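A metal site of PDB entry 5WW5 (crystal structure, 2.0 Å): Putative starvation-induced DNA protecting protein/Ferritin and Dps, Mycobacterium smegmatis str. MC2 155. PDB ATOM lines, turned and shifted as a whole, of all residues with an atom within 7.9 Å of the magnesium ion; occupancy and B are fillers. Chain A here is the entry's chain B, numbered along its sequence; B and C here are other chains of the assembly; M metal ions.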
ATOM      1  N   SER A  47     -12.533 -13.294  27.517  1.00  0.00           N
ATOM      2  CA  SER A  47     -13.528 -13.271  26.451  1.00  0.00           C
ATOM      3  C   SER A  47     -14.183 -14.637  26.274  1.00  0.00           C
ATOM      4  O   SER A  47     -13.498 -15.620  26.042  1.00  0.00           O
ATOM      5  CB  SER A  47     -12.884 -12.822  25.144  1.00  0.00           C
ATOM      6  OG  SER A  47     -12.240 -11.563  25.307  1.00  0.00           O
ATOM      7  N   ASN A  48     -15.510 -14.667  26.387  1.00  0.00           N
ATOM      8  CA  ASN A  48     -16.309 -15.900  26.290  1.00  0.00           C
ATOM      9  C   ASN A  48     -16.071 -16.909  27.434  1.00  0.00           C
ATOM     10  O   ASN A  48     -16.153 -18.129  27.235  1.00  0.00           O
ATOM     11  CB  ASN A  48     -16.177 -16.572  24.914  1.00  0.00           C
ATOM     12  CG  ASN A  48     -17.363 -17.446  24.593  1.00  0.00           C
ATOM     13  OD1 ASN A  48     -18.469 -17.185  25.068  1.00  0.00           O
ATOM     14  ND2 ASN A  48     -17.142 -18.493  23.800  1.00  0.00           N
ATOM     15  N   PHE A  49     -15.807 -16.367  28.618  1.00  0.00           N
ATOM     16  CA  PHE A  49     -15.653 -17.152  29.849  1.00  0.00           C
ATOM     17  C   PHE A  49     -16.763 -18.187  30.027  1.00  0.00           C
ATOM     18  O   PHE A  49     -16.486 -19.381  30.237  1.00  0.00           O
ATOM     19  CB  PHE A  49     -15.607 -16.222  31.075  1.00  0.00           C
ATOM     20  CG  PHE A  49     -15.937 -16.904  32.379  1.00  0.00           C
ATOM     21  CD1 PHE A  49     -14.979 -17.706  33.019  1.00  0.00           C
ATOM     22  CD2 PHE A  49     -17.196 -16.755  32.984  1.00  0.00           C
ATOM     23  CE1 PHE A  49     -15.276 -18.362  34.222  1.00  0.00           C
ATOM     24  CE2 PHE A  49     -17.498 -17.404  34.181  1.00  0.00           C
ATOM     25  CZ  PHE A  49     -16.546 -18.200  34.798  1.00  0.00           C
ATOM     26  N   ARG A  50     -18.012 -17.731  29.958  1.00  0.00           N
ATOM     27  CA  ARG A  50     -19.142 -18.537  30.407  1.00  0.00           C
ATOM     28  C   ARG A  50     -19.299 -19.826  29.593  1.00  0.00           C
ATOM     29  O   ARG A  50     -19.395 -20.904  30.168  1.00  0.00           O
ATOM     30  CB  ARG A  50     -20.420 -17.709  30.436  1.00  0.00           C
ATOM     31  CG  ARG A  50     -21.585 -18.440  31.089  1.00  0.00           C
ATOM     32  CD  ARG A  50     -22.830 -17.558  31.104  1.00  0.00           C
ATOM     33  NE  ARG A  50     -23.998 -18.273  31.604  1.00  0.00           N
ATOM     34  CZ  ARG A  50     -24.854 -18.981  30.867  1.00  0.00           C
ATOM     35  NH1 ARG A  50     -24.677 -19.124  29.561  1.00  0.00           N
ATOM     36  NH2 ARG A  50     -25.887 -19.579  31.468  1.00  0.00           N
ATOM     37  N   ASP A  51     -19.311 -19.694  28.257  1.00  0.00           N
ATOM     38  CA  ASP A  51     -19.360 -20.845  27.364  1.00  0.00           C
ATOM     39  C   ASP A  51     -18.281 -21.870  27.676  1.00  0.00           C
ATOM     40  O   ASP A  51     -18.559 -23.072  27.691  1.00  0.00           O
ATOM     41  CB  ASP A  51     -19.209 -20.418  25.900  1.00  0.00           C
ATOM     42  CG  ASP A  51     -20.518 -20.202  25.209  1.00  0.00           C
ATOM     43  OD1 ASP A  51     -21.498 -20.944  25.474  1.00  0.00           O
ATOM     44  OD2 ASP A  51     -20.578 -19.289  24.370  1.00  0.00           O
ATOM     45  N   LEU A  52     -17.051 -21.388  27.916  1.00  0.00           N
ATOM     46  CA  LEU A  52     -15.940 -22.287  28.231  1.00  0.00           C
ATOM     47  C   LEU A  52     -16.085 -22.951  29.584  1.00  0.00           C
ATOM     48  O   LEU A  52     -15.934 -24.155  29.690  1.00  0.00           O
ATOM     49  CB  LEU A  52     -14.579 -21.591  28.115  1.00  0.00           C
ATOM     50  CG  LEU A  52     -13.809 -21.808  26.806  1.00  0.00           C
ATOM     51  CD1 LEU A  52     -13.505 -23.288  26.567  1.00  0.00           C
ATOM     52  CD2 LEU A  52     -14.521 -21.161  25.612  1.00  0.00           C
ATOM     53  N   GLU A 157     -13.758 -22.508  19.105  1.00  0.00           N
ATOM     54  CA  GLU A 157     -13.617 -21.154  19.659  1.00  0.00           C
ATOM     55  C   GLU A 157     -12.385 -20.389  19.117  1.00  0.00           C
ATOM     56  O   GLU A 157     -12.463 -19.184  18.883  1.00  0.00           O
ATOM     57  CB  GLU A 157     -13.563 -21.236  21.196  1.00  0.00           C
ATOM     58  CG  GLU A 157     -13.224 -19.958  21.956  1.00  0.00           C
ATOM     59  CD  GLU A 157     -14.288 -18.873  21.859  1.00  0.00           C
ATOM     60  OE1 GLU A 157     -13.928 -17.688  22.022  1.00  0.00           O
ATOM     61  OE2 GLU A 157     -15.482 -19.199  21.638  1.00  0.00           O
ATOM     62  N   SER B  47     -14.744 -17.112  17.333  1.00  0.00           N
ATOM     63  CA  SER B  47     -15.077 -16.434  18.597  1.00  0.00           C
ATOM     64  C   SER B  47     -16.556 -16.560  18.926  1.00  0.00           C
ATOM     65  O   SER B  47     -17.419 -16.238  18.111  1.00  0.00           O
ATOM     66  CB  SER B  47     -14.650 -14.971  18.547  1.00  0.00           C
ATOM     67  OG  SER B  47     -13.245 -14.868  18.405  1.00  0.00           O
ATOM     68  N   ASN B  48     -16.828 -17.060  20.138  1.00  0.00           N
ATOM     69  CA  ASN B  48     -18.184 -17.348  20.649  1.00  0.00           C
ATOM     70  C   ASN B  48     -18.940 -18.446  19.875  1.00  0.00           C
ATOM     71  O   ASN B  48     -20.164 -18.396  19.722  1.00  0.00           O
ATOM     72  CB  ASN B  48     -19.027 -16.064  20.822  1.00  0.00           C
ATOM     73  CG  ASN B  48     -20.152 -16.235  21.830  1.00  0.00           C
ATOM     74  OD1 ASN B  48     -20.037 -17.036  22.758  1.00  0.00           O
ATOM     75  ND2 ASN B  48     -21.246 -15.511  21.642  1.00  0.00           N
ATOM     76  N   PHE B  49     -18.182 -19.453  19.401  1.00  0.00           N
ATOM     77  CA  PHE B  49     -18.712 -20.631  18.718  1.00  0.00           C
ATOM     78  C   PHE B  49     -19.896 -21.284  19.444  1.00  0.00           C
ATOM     79  O   PHE B  49     -20.923 -21.543  18.820  1.00  0.00           O
ATOM     80  CB  PHE B  49     -17.615 -21.700  18.511  1.00  0.00           C
ATOM     81  CG  PHE B  49     -18.166 -23.086  18.228  1.00  0.00           C
ATOM     82  CD1 PHE B  49     -18.244 -24.043  19.248  1.00  0.00           C
ATOM     83  CD2 PHE B  49     -18.619 -23.422  16.949  1.00  0.00           C
ATOM     84  CE1 PHE B  49     -18.762 -25.315  18.986  1.00  0.00           C
ATOM     85  CE2 PHE B  49     -19.141 -24.687  16.681  1.00  0.00           C
ATOM     86  CZ  PHE B  49     -19.214 -25.637  17.706  1.00  0.00           C
ATOM     87  N   ARG B  50     -19.719 -21.547  20.738  1.00  0.00           N
ATOM     88  CA  ARG B  50     -20.698 -22.355  21.482  1.00  0.00           C
ATOM     89  C   ARG B  50     -22.081 -21.711  21.569  1.00  0.00           C
ATOM     90  O   ARG B  50     -23.082 -22.378  21.259  1.00  0.00           O
ATOM     91  CB  ARG B  50     -20.155 -22.717  22.871  1.00  0.00           C
ATOM     92  CG  ARG B  50     -21.033 -23.675  23.654  1.00  0.00           C
ATOM     93  CD  ARG B  50     -20.343 -24.072  24.955  1.00  0.00           C
ATOM     94  NE  ARG B  50     -21.187 -24.966  25.751  1.00  0.00           N
ATOM     95  CZ  ARG B  50     -22.140 -24.561  26.591  1.00  0.00           C
ATOM     96  NH1 ARG B  50     -22.410 -23.265  26.758  1.00  0.00           N
ATOM     97  NH2 ARG B  50     -22.854 -25.471  27.264  1.00  0.00           N
ATOM     98  N   ASP B  51     -22.137 -20.441  21.953  1.00  0.00           N
ATOM     99  CA  ASP B  51     -23.394 -19.690  22.014  1.00  0.00           C
ATOM    100  C   ASP B  51     -24.151 -19.761  20.700  1.00  0.00           C
ATOM    101  O   ASP B  51     -25.355 -19.999  20.677  1.00  0.00           O
ATOM    102  CB  ASP B  51     -23.143 -18.230  22.364  1.00  0.00           C
ATOM    103  CG  ASP B  51     -23.254 -17.947  23.855  1.00  0.00           C
ATOM    104  OD1 ASP B  51     -24.137 -18.545  24.528  1.00  0.00           O
ATOM    105  OD2 ASP B  51     -22.487 -17.092  24.347  1.00  0.00           O
ATOM    106  N   LEU B  52     -23.430 -19.548  19.593  1.00  0.00           N
ATOM    107  CA  LEU B  52     -24.015 -19.571  18.251  1.00  0.00           C
ATOM    108  C   LEU B  52     -24.460 -20.971  17.848  1.00  0.00           C
ATOM    109  O   LEU B  52     -25.576 -21.142  17.381  1.00  0.00           O
ATOM    110  CB  LEU B  52     -23.048 -18.977  17.227  1.00  0.00           C
ATOM    111  CG  LEU B  52     -23.280 -17.516  16.826  1.00  0.00           C
ATOM    112  CD1 LEU B  52     -24.670 -17.306  16.211  1.00  0.00           C
ATOM    113  CD2 LEU B  52     -23.049 -16.583  18.014  1.00  0.00           C
ATOM    114  N   GLU B 157     -25.126 -10.364  18.719  1.00  0.00           N
ATOM    115  CA  GLU B 157     -23.699 -10.718  18.731  1.00  0.00           C
ATOM    116  C   GLU B 157     -22.801  -9.754  17.940  1.00  0.00           C
ATOM    117  O   GLU B 157     -21.691  -9.471  18.370  1.00  0.00           O
ATOM    118  CB  GLU B 157     -23.515 -12.147  18.195  1.00  0.00           C
ATOM    119  CG  GLU B 157     -22.070 -12.630  18.023  1.00  0.00           C
ATOM    120  CD  GLU B 157     -21.272 -12.754  19.317  1.00  0.00           C
ATOM    121  OE1 GLU B 157     -21.836 -13.062  20.397  1.00  0.00           O
ATOM    122  OE2 GLU B 157     -20.040 -12.553  19.257  1.00  0.00           O
ATOM    123  N   SER C  47     -20.398  -8.509  21.453  1.00  0.00           N
ATOM    124  CA  SER C  47     -19.650  -9.767  21.543  1.00  0.00           C
ATOM    125  C   SER C  47     -20.025 -10.537  22.795  1.00  0.00           C
ATOM    126  O   SER C  47     -19.998  -9.999  23.902  1.00  0.00           O
ATOM    127  CB  SER C  47     -18.148  -9.480  21.525  1.00  0.00           C
ATOM    128  OG  SER C  47     -17.409 -10.684  21.496  1.00  0.00           O
ATOM    129  N   ASN C  48     -20.383 -11.808  22.616  1.00  0.00           N
ATOM    130  CA  ASN C  48     -20.825 -12.696  23.694  1.00  0.00           C
ATOM    131  C   ASN C  48     -22.151 -12.277  24.340  1.00  0.00           C
ATOM    132  O   ASN C  48     -22.385 -12.510  25.543  1.00  0.00           O
ATOM    133  CB  ASN C  48     -19.722 -12.929  24.755  1.00  0.00           C
ATOM    134  CG  ASN C  48     -19.884 -14.257  25.453  1.00  0.00           C
ATOM    135  OD1 ASN C  48     -20.467 -15.182  24.887  1.00  0.00           O
ATOM    136  ND2 ASN C  48     -19.390 -14.360  26.683  1.00  0.00           N
ATOM    137  N   PHE C  49     -23.013 -11.642  23.530  1.00  0.00           N
ATOM    138  CA  PHE C  49     -24.364 -11.256  23.948  1.00  0.00           C
ATOM    139  C   PHE C  49     -25.086 -12.396  24.670  1.00  0.00           C
ATOM    140  O   PHE C  49     -25.624 -12.192  25.759  1.00  0.00           O
ATOM    141  CB  PHE C  49     -25.219 -10.789  22.741  1.00  0.00           C
ATOM    142  CG  PHE C  49     -26.697 -10.873  22.979  1.00  0.00           C
ATOM    143  CD1 PHE C  49     -27.358  -9.898  23.723  1.00  0.00           C
ATOM    144  CD2 PHE C  49     -27.437 -11.962  22.501  1.00  0.00           C
ATOM    145  CE1 PHE C  49     -28.732  -9.993  23.971  1.00  0.00           C
ATOM    146  CE2 PHE C  49     -28.799 -12.065  22.747  1.00  0.00           C
ATOM    147  CZ  PHE C  49     -29.452 -11.077  23.483  1.00  0.00           C
ATOM    148  N   ARG C  50     -25.128 -13.574  24.053  1.00  0.00           N
ATOM    149  CA  ARG C  50     -26.001 -14.659  24.505  1.00  0.00           C
ATOM    150  C   ARG C  50     -25.661 -15.131  25.925  1.00  0.00           C
ATOM    151  O   ARG C  50     -26.550 -15.203  26.776  1.00  0.00           O
ATOM    152  CB  ARG C  50     -26.004 -15.828  23.501  1.00  0.00           C
ATOM    153  CG  ARG C  50     -26.996 -16.930  23.872  1.00  0.00           C
ATOM    154  CD  ARG C  50     -26.995 -18.051  22.853  1.00  0.00           C
ATOM    155  NE  ARG C  50     -27.944 -19.111  23.220  1.00  0.00           N
ATOM    156  CZ  ARG C  50     -27.654 -20.177  23.957  1.00  0.00           C
ATOM    157  NH1 ARG C  50     -26.434 -20.348  24.459  1.00  0.00           N
ATOM    158  NH2 ARG C  50     -28.593 -21.077  24.211  1.00  0.00           N
ATOM    159  N   ASP C  51     -24.374 -15.410  26.175  1.00  0.00           N
ATOM    160  CA  ASP C  51     -23.878 -15.760  27.512  1.00  0.00           C
ATOM    161  C   ASP C  51     -24.299 -14.761  28.582  1.00  0.00           C
ATOM    162  O   ASP C  51     -24.797 -15.158  29.642  1.00  0.00           O
ATOM    163  CB  ASP C  51     -22.359 -15.883  27.535  1.00  0.00           C
ATOM    164  CG  ASP C  51     -21.866 -17.297  27.328  1.00  0.00           C
ATOM    165  OD1 ASP C  51     -22.509 -18.245  27.831  1.00  0.00           O
ATOM    166  OD2 ASP C  51     -20.833 -17.458  26.645  1.00  0.00           O
ATOM    167  N   LEU C  52     -24.109 -13.472  28.287  1.00  0.00           N
ATOM    168  CA  LEU C  52     -24.478 -12.414  29.228  1.00  0.00           C
ATOM    169  C   LEU C  52     -25.976 -12.275  29.417  1.00  0.00           C
ATOM    170  O   LEU C  52     -26.434 -12.135  30.541  1.00  0.00           O
ATOM    171  CB  LEU C  52     -23.812 -11.072  28.862  1.00  0.00           C
ATOM    172  CG  LEU C  52     -22.466 -10.785  29.544  1.00  0.00           C
ATOM    173  CD1 LEU C  52     -22.628 -10.739  31.055  1.00  0.00           C
ATOM    174  CD2 LEU C  52     -21.388 -11.791  29.148  1.00  0.00           C
ATOM    175  N   GLU C 157     -15.694 -12.419  32.299  1.00  0.00           N
ATOM    176  CA  GLU C 157     -15.737 -12.037  30.884  1.00  0.00           C
ATOM    177  C   GLU C 157     -14.740 -10.928  30.517  1.00  0.00           C
ATOM    178  O   GLU C 157     -14.142 -10.962  29.442  1.00  0.00           O
ATOM    179  CB  GLU C 157     -17.163 -11.614  30.497  1.00  0.00           C
ATOM    180  CG  GLU C 157     -17.336 -10.968  29.115  1.00  0.00           C
ATOM    181  CD  GLU C 157     -17.040 -11.900  27.946  1.00  0.00           C
ATOM    182  OE1 GLU C 157     -16.633 -11.393  26.879  1.00  0.00           O
ATOM    183  OE2 GLU C 157     -17.201 -13.133  28.075  1.00  0.00           O
HETATM  184 MG    MG M   1     -20.427 -17.218  24.669  1.00  0.00          MG
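Of the 21 residues printed, 6 come within 4 Å of the magnesium ion. The nearest printed residue that does not touch the magnesium ion is Arg 50 of chain A (5.7 Å).
ND2 of Asn 48 of chain B sits at hydrogen-bond distance from OE1 of Glu 157 of chain B, 2.8 Å away. The side-chain carboxylate (OE2) of Glu 157 of chain A is in hydrogen-bond range of the backbone NH (N) of Asn 48 of chain B, 2.9 Å away. OE2 of Glu 157 of chain A sits at hydrogen-bond distance from ND2 of Asn 48 of chain A, at 2.8 Å. N of Asn 48 of chain A is in hydrogen-bond range of OE2 of Glu 157 of chain C (2.8 Å). The backbone NH (N) of Asn 48 of chain C lies within hydrogen-bond range of the side-chain carboxylate (OE1) of Glu 157 of chain B. The side-chain carboxylate (OE2) of Glu 157 of chain C lies within hydrogen-bond range of the side-chain amide nitrogen (ND2) of Asn 48 of chain C (2.9 Å). OD1 of Asp 51 of chain B lies within salt-bridge range of NH1 of Arg 50 of chain C, at 2.9 Å. The guanidinium group (NH1) of Arg 50 of chain B is in salt-bridge range of the side-chain carboxylate (OD1) of Asp 51 of chain A.
The magnesium ion is bound by OD1 of Asn 48 of chain B (2.0 Å), OD1 of Asn 48 of chain A (2.0 Å), OD2 of Asp 51 of chain C (2.0 Å), OD1 of Asn 48 of chain C (2.0 Å), OD2 of Asp 51 of chain B (2.1 Å) and OD2 of Asp 51 of chain A (2.1 Å). The magnesium ion has six donor atoms within binding distance.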
